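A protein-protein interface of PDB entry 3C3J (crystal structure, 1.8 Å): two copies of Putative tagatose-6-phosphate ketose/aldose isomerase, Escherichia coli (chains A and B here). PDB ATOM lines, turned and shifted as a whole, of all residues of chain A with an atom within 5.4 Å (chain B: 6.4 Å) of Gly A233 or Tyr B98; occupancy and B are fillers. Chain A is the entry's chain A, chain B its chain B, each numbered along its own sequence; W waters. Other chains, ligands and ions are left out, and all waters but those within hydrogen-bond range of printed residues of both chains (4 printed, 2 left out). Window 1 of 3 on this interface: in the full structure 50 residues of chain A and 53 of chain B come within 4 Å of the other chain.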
ATOM      1  N   ASP A  69      -6.895  24.807  20.271  1.00  0.00           N
ATOM      2  CA  ASP A  69      -7.870  25.909  20.345  1.00  0.00           C
ATOM      3  C   ASP A  69      -7.721  26.885  19.185  1.00  0.00           C
ATOM      4  O   ASP A  69      -8.732  27.346  18.623  1.00  0.00           O
ATOM      5  CB  ASP A  69      -7.783  26.650  21.669  1.00  0.00           C
ATOM      6  CG  ASP A  69      -8.252  25.802  22.864  1.00  0.00           C
ATOM      7  OD1 ASP A  69      -8.882  24.750  22.665  1.00  0.00           O
ATOM      8  OD2 ASP A  69      -7.971  26.192  24.020  1.00  0.00           O
ATOM      9  N   PRO A  73     -10.345  24.123  14.546  1.00  0.00           N
ATOM     10  CA  PRO A  73     -11.480  24.460  13.681  1.00  0.00           C
ATOM     11  C   PRO A  73     -11.068  24.775  12.257  1.00  0.00           C
ATOM     12  O   PRO A  73     -11.686  24.275  11.331  1.00  0.00           O
ATOM     13  CB  PRO A  73     -12.087  25.692  14.354  1.00  0.00           C
ATOM     14  CG  PRO A  73     -11.601  25.605  15.792  1.00  0.00           C
ATOM     15  CD  PRO A  73     -10.229  25.072  15.669  1.00  0.00           C
ATOM     16  N   GLY A 231     -10.023  37.914  20.835  1.00  0.00           N
ATOM     17  CA  GLY A 231      -9.829  37.441  19.463  1.00  0.00           C
ATOM     18  C   GLY A 231     -10.992  36.557  19.047  1.00  0.00           C
ATOM     19  O   GLY A 231     -11.501  35.791  19.858  1.00  0.00           O
ATOM     20  N   SER A 232     -11.404  36.659  17.790  1.00  0.00           N
ATOM     21  CA  SER A 232     -12.545  35.894  17.289  1.00  0.00           C
ATOM     22  C   SER A 232     -12.126  34.512  16.821  1.00  0.00           C
ATOM     23  O   SER A 232     -10.996  34.304  16.355  1.00  0.00           O
ATOM     24  CB  SER A 232     -13.262  36.626  16.134  1.00  0.00           C
ATOM     25  OG  SER A 232     -13.878  37.827  16.566  1.00  0.00           O
ATOM     26  N   GLY A 233     -13.034  33.554  16.948  1.00  0.00           N
ATOM     27  CA  GLY A 233     -12.785  32.209  16.414  1.00  0.00           C
ATOM     28  C   GLY A 233     -11.573  31.614  17.087  1.00  0.00           C
ATOM     29  O   GLY A 233     -11.415  31.733  18.312  1.00  0.00           O
ATOM     30  N   GLY A 234     -10.669  31.046  16.287  1.00  0.00           N
ATOM     31  CA  GLY A 234      -9.429  30.485  16.797  1.00  0.00           C
ATOM     32  C   GLY A 234      -8.455  31.481  17.428  1.00  0.00           C
ATOM     33  O   GLY A 234      -7.612  31.092  18.222  1.00  0.00           O
ATOM     34  N   LEU A 235      -8.569  32.768  17.094  1.00  0.00           N
ATOM     35  CA  LEU A 235      -7.742  33.772  17.756  1.00  0.00           C
ATOM     36  C   LEU A 235      -8.080  33.944  19.222  1.00  0.00           C
ATOM     37  O   LEU A 235      -7.290  34.518  19.970  1.00  0.00           O
ATOM     38  CB  LEU A 235      -7.812  35.119  17.058  1.00  0.00           C
ATOM     39  CG  LEU A 235      -7.220  35.190  15.656  1.00  0.00           C
ATOM     40  CD1 LEU A 235      -7.512  36.571  15.045  1.00  0.00           C
ATOM     41  CD2 LEU A 235      -5.707  34.866  15.648  1.00  0.00           C
ATOM     42  N   GLN A 236      -9.244  33.455  19.650  1.00  0.00           N
ATOM     43  CA  GLN A 236      -9.528  33.392  21.067  1.00  0.00           C
ATOM     44  C   GLN A 236      -8.476  32.509  21.784  1.00  0.00           C
ATOM     45  O   GLN A 236      -8.056  32.813  22.916  1.00  0.00           O
ATOM     46  CB  GLN A 236     -10.965  32.935  21.376  1.00  0.00           C
ATOM     47  CG  GLN A 236     -11.220  33.043  22.874  1.00  0.00           C
ATOM     48  CD  GLN A 236     -12.600  32.673  23.351  1.00  0.00           C
ATOM     49  OE1 GLN A 236     -13.529  32.332  22.563  1.00  0.00           O
ATOM     50  NE2 GLN A 236     -12.751  32.714  24.680  1.00  0.00           N
ATOM     51  N   GLY A 237      -8.046  31.426  21.134  1.00  0.00           N
ATOM     52  CA  GLY A 237      -6.966  30.603  21.683  1.00  0.00           C
ATOM     53  C   GLY A 237      -5.649  31.360  21.831  1.00  0.00           C
ATOM     54  O   GLY A 237      -4.912  31.151  22.792  1.00  0.00           O
ATOM     55  N   SER A 260     -13.734  36.173  23.187  1.00  0.00           N
ATOM     56  CA  SER A 260     -13.934  36.645  21.832  1.00  0.00           C
ATOM     57  C   SER A 260     -14.589  38.024  21.928  1.00  0.00           C
ATOM     58  O   SER A 260     -15.241  38.321  22.916  1.00  0.00           O
ATOM     59  CB  SER A 260     -14.833  35.714  21.042  1.00  0.00           C
ATOM     60  OG  SER A 260     -16.119  35.715  21.587  1.00  0.00           O
ATOM     61  N   ILE B  57     -25.313  20.385  17.137  1.00  0.00           N
ATOM     62  CA  ILE B  57     -24.549  21.430  17.755  1.00  0.00           C
ATOM     63  C   ILE B  57     -25.443  22.158  18.717  1.00  0.00           C
ATOM     64  O   ILE B  57     -26.519  22.623  18.331  1.00  0.00           O
ATOM     65  CB  ILE B  57     -23.985  22.440  16.711  1.00  0.00           C
ATOM     66  CG1 ILE B  57     -22.947  21.760  15.828  1.00  0.00           C
ATOM     67  CG2 ILE B  57     -23.339  23.698  17.426  1.00  0.00           C
ATOM     68  CD1 ILE B  57     -22.530  22.608  14.583  1.00  0.00           C
ATOM     69  N   VAL B  86     -20.907  24.770  20.345  1.00  0.00           N
ATOM     70  CA  VAL B  86     -20.252  25.932  19.746  1.00  0.00           C
ATOM     71  C   VAL B  86     -21.084  27.172  20.090  1.00  0.00           C
ATOM     72  O   VAL B  86     -22.258  27.234  19.753  1.00  0.00           O
ATOM     73  CB  VAL B  86     -20.173  25.848  18.214  1.00  0.00           C
ATOM     74  CG1 VAL B  86     -19.385  27.022  17.673  1.00  0.00           C
ATOM     75  CG2 VAL B  86     -19.538  24.490  17.744  1.00  0.00           C
ATOM     76  N   PRO B  87     -20.483  28.173  20.712  1.00  0.00           N
ATOM     77  CA  PRO B  87     -21.294  29.361  21.003  1.00  0.00           C
ATOM     78  C   PRO B  87     -21.810  30.075  19.761  1.00  0.00           C
ATOM     79  O   PRO B  87     -21.145  30.075  18.712  1.00  0.00           O
ATOM     80  CB  PRO B  87     -20.340  30.272  21.777  1.00  0.00           C
ATOM     81  CG  PRO B  87     -19.231  29.369  22.229  1.00  0.00           C
ATOM     82  CD  PRO B  87     -19.113  28.291  21.233  1.00  0.00           C
ATOM     83  N   THR B  89     -21.841  33.077  19.354  1.00  0.00           N
ATOM     84  CA  THR B  89     -20.901  34.167  19.132  1.00  0.00           C
ATOM     85  C   THR B  89     -19.760  33.724  18.201  1.00  0.00           C
ATOM     86  O   THR B  89     -19.302  34.515  17.377  1.00  0.00           O
ATOM     87  CB  THR B  89     -20.415  34.732  20.495  1.00  0.00           C
ATOM     88  OG1 THR B  89     -20.030  33.659  21.357  1.00  0.00           O
ATOM     89  CG2 THR B  89     -21.540  35.543  21.165  1.00  0.00           C
ATOM     90  N   ASP B  90     -19.370  32.445  18.253  1.00  0.00           N
ATOM     91  CA  ASP B  90     -18.402  31.883  17.310  1.00  0.00           C
ATOM     92  C   ASP B  90     -19.058  31.514  15.977  1.00  0.00           C
ATOM     93  O   ASP B  90     -18.453  31.719  14.934  1.00  0.00           O
ATOM     94  CB  ASP B  90     -17.733  30.623  17.870  1.00  0.00           C
ATOM     95  CG  ASP B  90     -16.814  30.907  19.057  1.00  0.00           C
ATOM     96  OD1 ASP B  90     -16.336  32.066  19.224  1.00  0.00           O
ATOM     97  OD2 ASP B  90     -16.556  29.942  19.816  1.00  0.00           O
ATOM     98  N   LEU B  91     -20.270  30.956  15.992  1.00  0.00           N
ATOM     99  CA  LEU B  91     -20.972  30.653  14.735  1.00  0.00           C
ATOM    100  C   LEU B  91     -21.163  31.917  13.897  1.00  0.00           C
ATOM    101  O   LEU B  91     -21.041  31.872  12.675  1.00  0.00           O
ATOM    102  CB  LEU B  91     -22.343  30.000  14.983  1.00  0.00           C
ATOM    103  CG  LEU B  91     -22.380  28.569  15.521  1.00  0.00           C
ATOM    104  CD1 LEU B  91     -23.826  28.083  15.681  1.00  0.00           C
ATOM    105  CD2 LEU B  91     -21.570  27.618  14.617  1.00  0.00           C
ATOM    106  N   THR B  93     -19.392  34.856  13.923  1.00  0.00           N
ATOM    107  CA  THR B  93     -18.170  35.504  13.427  1.00  0.00           C
ATOM    108  C   THR B  93     -17.363  34.597  12.501  1.00  0.00           C
ATOM    109  O   THR B  93     -16.689  35.076  11.614  1.00  0.00           O
ATOM    110  CB  THR B  93     -17.254  35.928  14.562  1.00  0.00           C
ATOM    111  OG1 THR B  93     -16.789  34.759  15.239  1.00  0.00           O
ATOM    112  CG2 THR B  93     -17.971  36.930  15.553  1.00  0.00           C
ATOM    113  N   ASN B  94     -17.455  33.283  12.698  1.00  0.00           N
ATOM    114  CA  ASN B  94     -16.606  32.290  11.992  1.00  0.00           C
ATOM    115  C   ASN B  94     -17.402  31.083  11.515  1.00  0.00           C
ATOM    116  O   ASN B  94     -17.038  29.943  11.787  1.00  0.00           O
ATOM    117  CB  ASN B  94     -15.488  31.786  12.911  1.00  0.00           C
ATOM    118  CG  ASN B  94     -14.390  32.811  13.148  1.00  0.00           C
ATOM    119  OD1 ASN B  94     -13.279  32.685  12.596  1.00  0.00           O
ATOM    120  ND2 ASN B  94     -14.667  33.811  13.975  1.00  0.00           N
ATOM    121  N   PRO B  95     -18.498  31.326  10.795  1.00  0.00           N
ATOM    122  CA  PRO B  95     -19.405  30.235  10.448  1.00  0.00           C
ATOM    123  C   PRO B  95     -18.708  29.131   9.676  1.00  0.00           C
ATOM    124  O   PRO B  95     -18.968  27.935   9.925  1.00  0.00           O
ATOM    125  CB  PRO B  95     -20.482  30.930   9.594  1.00  0.00           C
ATOM    126  CG  PRO B  95     -19.858  32.133   9.085  1.00  0.00           C
ATOM    127  CD  PRO B  95     -18.952  32.602  10.224  1.00  0.00           C
ATOM    128  N   MET B  96     -17.786  29.538   8.802  1.00  0.00           N
ATOM    129  CA  MET B  96     -17.046  28.605   7.936  1.00  0.00           C
ATOM    130  C   MET B  96     -16.193  27.610   8.718  1.00  0.00           C
ATOM    131  O   MET B  96     -15.892  26.538   8.210  1.00  0.00           O
ATOM    132  CB  MET B  96     -16.169  29.369   6.917  1.00  0.00           C
ATOM    133  CG  MET B  96     -15.065  30.249   7.524  1.00  0.00           C
ATOM    134  SD  MET B  96     -15.657  32.063   8.165  1.00  0.00           S
ATOM    135  CE  MET B  96     -13.992  32.577   9.124  1.00  0.00           C
ATOM    136  N   ASP B  97     -15.796  27.973   9.939  1.00  0.00           N
ATOM    137  CA  ASP B  97     -14.997  27.090  10.778  1.00  0.00           C
ATOM    138  C   ASP B  97     -15.784  25.980  11.473  1.00  0.00           C
ATOM    139  O   ASP B  97     -15.188  25.025  11.980  1.00  0.00           O
ATOM    140  CB  ASP B  97     -14.240  27.901  11.817  1.00  0.00           C
ATOM    141  CG  ASP B  97     -13.188  28.816  11.208  1.00  0.00           C
ATOM    142  OD1 ASP B  97     -12.804  28.654  10.025  1.00  0.00           O
ATOM    143  OD2 ASP B  97     -12.715  29.706  11.939  1.00  0.00           O
ATOM    144  N   TYR B  98     -17.116  26.103  11.528  1.00  0.00           N
ATOM    145  CA  TYR B  98     -17.933  25.191  12.345  1.00  0.00           C
ATOM    146  C   TYR B  98     -19.085  24.525  11.613  1.00  0.00           C
ATOM    147  O   TYR B  98     -19.553  23.478  12.043  1.00  0.00           O
ATOM    148  CB  TYR B  98     -18.506  25.938  13.555  1.00  0.00           C
ATOM    149  CG  TYR B  98     -17.468  26.652  14.360  1.00  0.00           C
ATOM    150  CD1 TYR B  98     -16.626  25.966  15.216  1.00  0.00           C
ATOM    151  CD2 TYR B  98     -17.328  28.013  14.268  1.00  0.00           C
ATOM    152  CE1 TYR B  98     -15.642  26.647  15.955  1.00  0.00           C
ATOM    153  CE2 TYR B  98     -16.356  28.686  14.976  1.00  0.00           C
ATOM    154  CZ  TYR B  98     -15.516  27.996  15.834  1.00  0.00           C
ATOM    155  OH  TYR B  98     -14.539  28.684  16.555  1.00  0.00           O
ATOM    156  N   LEU B  99     -19.592  25.147  10.552  1.00  0.00           N
ATOM    157  CA  LEU B  99     -20.758  24.623   9.866  1.00  0.00           C
ATOM    158  C   LEU B  99     -20.283  23.807   8.653  1.00  0.00           C
ATOM    159  O   LEU B  99     -19.688  24.355   7.718  1.00  0.00           O
ATOM    160  CB  LEU B  99     -21.702  25.753   9.444  1.00  0.00           C
ATOM    161  CG  LEU B  99     -22.281  26.617  10.577  1.00  0.00           C
ATOM    162  CD1 LEU B  99     -22.893  27.926  10.071  1.00  0.00           C
ATOM    163  CD2 LEU B  99     -23.289  25.830  11.384  1.00  0.00           C
ATOM    164  N   ASN B 100     -20.571  22.513   8.652  1.00  0.00           N
ATOM    165  CA  ASN B 100     -20.087  21.616   7.618  1.00  0.00           C
ATOM    166  C   ASN B 100     -21.182  21.286   6.598  1.00  0.00           C
ATOM    167  O   ASN B 100     -22.114  20.549   6.899  1.00  0.00           O
ATOM    168  CB  ASN B 100     -19.522  20.344   8.258  1.00  0.00           C
ATOM    169  CG  ASN B 100     -18.800  19.446   7.269  1.00  0.00           C
ATOM    170  OD1 ASN B 100     -19.000  19.515   6.048  1.00  0.00           O
ATOM    171  ND2 ASN B 100     -17.929  18.600   7.801  1.00  0.00           N
ATOM    172  N   LEU B 105     -27.195  18.676   9.752  1.00  0.00           N
ATOM    173  CA  LEU B 105     -27.009  19.361  11.033  1.00  0.00           C
ATOM    174  C   LEU B 105     -28.338  19.487  11.751  1.00  0.00           C
ATOM    175  O   LEU B 105     -29.354  19.816  11.141  1.00  0.00           O
ATOM    176  CB  LEU B 105     -26.440  20.748  10.785  1.00  0.00           C
ATOM    177  CG  LEU B 105     -26.298  21.693  11.983  1.00  0.00           C
ATOM    178  CD1 LEU B 105     -25.370  21.114  13.088  1.00  0.00           C
ATOM    179  CD2 LEU B 105     -25.839  23.084  11.542  1.00  0.00           C
HETATM  180  O   HOH W   1     -15.708  34.513  17.898  1.00  0.00           O
HETATM  181  O   HOH W   2     -15.434  29.732  22.222  1.00  0.00           O
HETATM  182  O   HOH W   3     -10.667  34.161  13.593  1.00  0.00           O
HETATM  183  O   HOH W   4     -17.393  33.172  21.274  1.00  0.00           O
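N of Gly A233 sits close to ND2 of Asn B94 (3.4 Å).
The side-chain amide oxygen (OD1) of Asn B94 sits close to the side-chain carboxylate (OD2) of Asp B97 (3.1 Å).
ND2 of Asn B94 is in hydrogen-bond range of OG1 of Thr B93, at 2.6 Å.
Among the printed residues, merely in contact across the chains: Pro A73 with Asp B97 (3.6 Å), Ser A232 with Asn B94 (3.8 Å) and Gly A233 with Tyr B98 (3.9 Å).
Of chain B, only Asn B94 and Tyr B98 come within 4 Å of Gly A233.
Of the printed residues of chain A, Tyr B98 touches Gly A233 (3.9 Å).
Of the printed residues of chain A, Asn B94 touches Ser A232 and Gly A233.
Printed residues of chain B within 4 Å of Pro A73: Asp B97.
Of the printed residues of chain B, Ser A232 touches Asn B94 (3.8 Å).
Of the printed residues of chain A, Asp B97 touches Pro A73.
Leu B91 touches none of the printed residues of chain A.
Met B96 touches none of the printed residues of chain A.
The nearest printed residue of chain B that does not touch Gly A233 is Asp B90 (4.3 Å).
The nearest printed residue of chain A that does not touch Asp B97 is Gly A234 (5.0 Å).
Among the printed residues, 4 pairs touch across the chains.
Among the printed residues, no Asp or Glu carboxylate lies within 4 Å of a Lys or Arg side-chain nitrogen of the other chain.
No position is printed for both chains.
Of the 4 pairs that touch across the chains among the printed residues, none has its exchanged pair printed and touching as well.
Water W4 lies within hydrogen-bond range of the side-chain carboxylate of Asp B90 (2.6 Å), the side-chain hydroxyl of Thr B89 (2.7 Å) and the side-chain hydroxyl of Ser A260 (2.9 Å).
Water W2 bridges OD2 of Asp B90 (2.7 Å) and OE1 of Gln A236 (3.2 Å).
Water W3 bridges O of Ser A232 (2.8 Å) and OD1 of Asn B94 (3.2 Å).
Water W1 lies within hydrogen-bond range of the side-chain carboxylate (OD1) of Asp B90 (2.9 Å), the side-chain hydroxyl (OG1) of Thr B93 (2.9 Å) and the backbone NH (N) of Gly A233 (3.0 Å).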
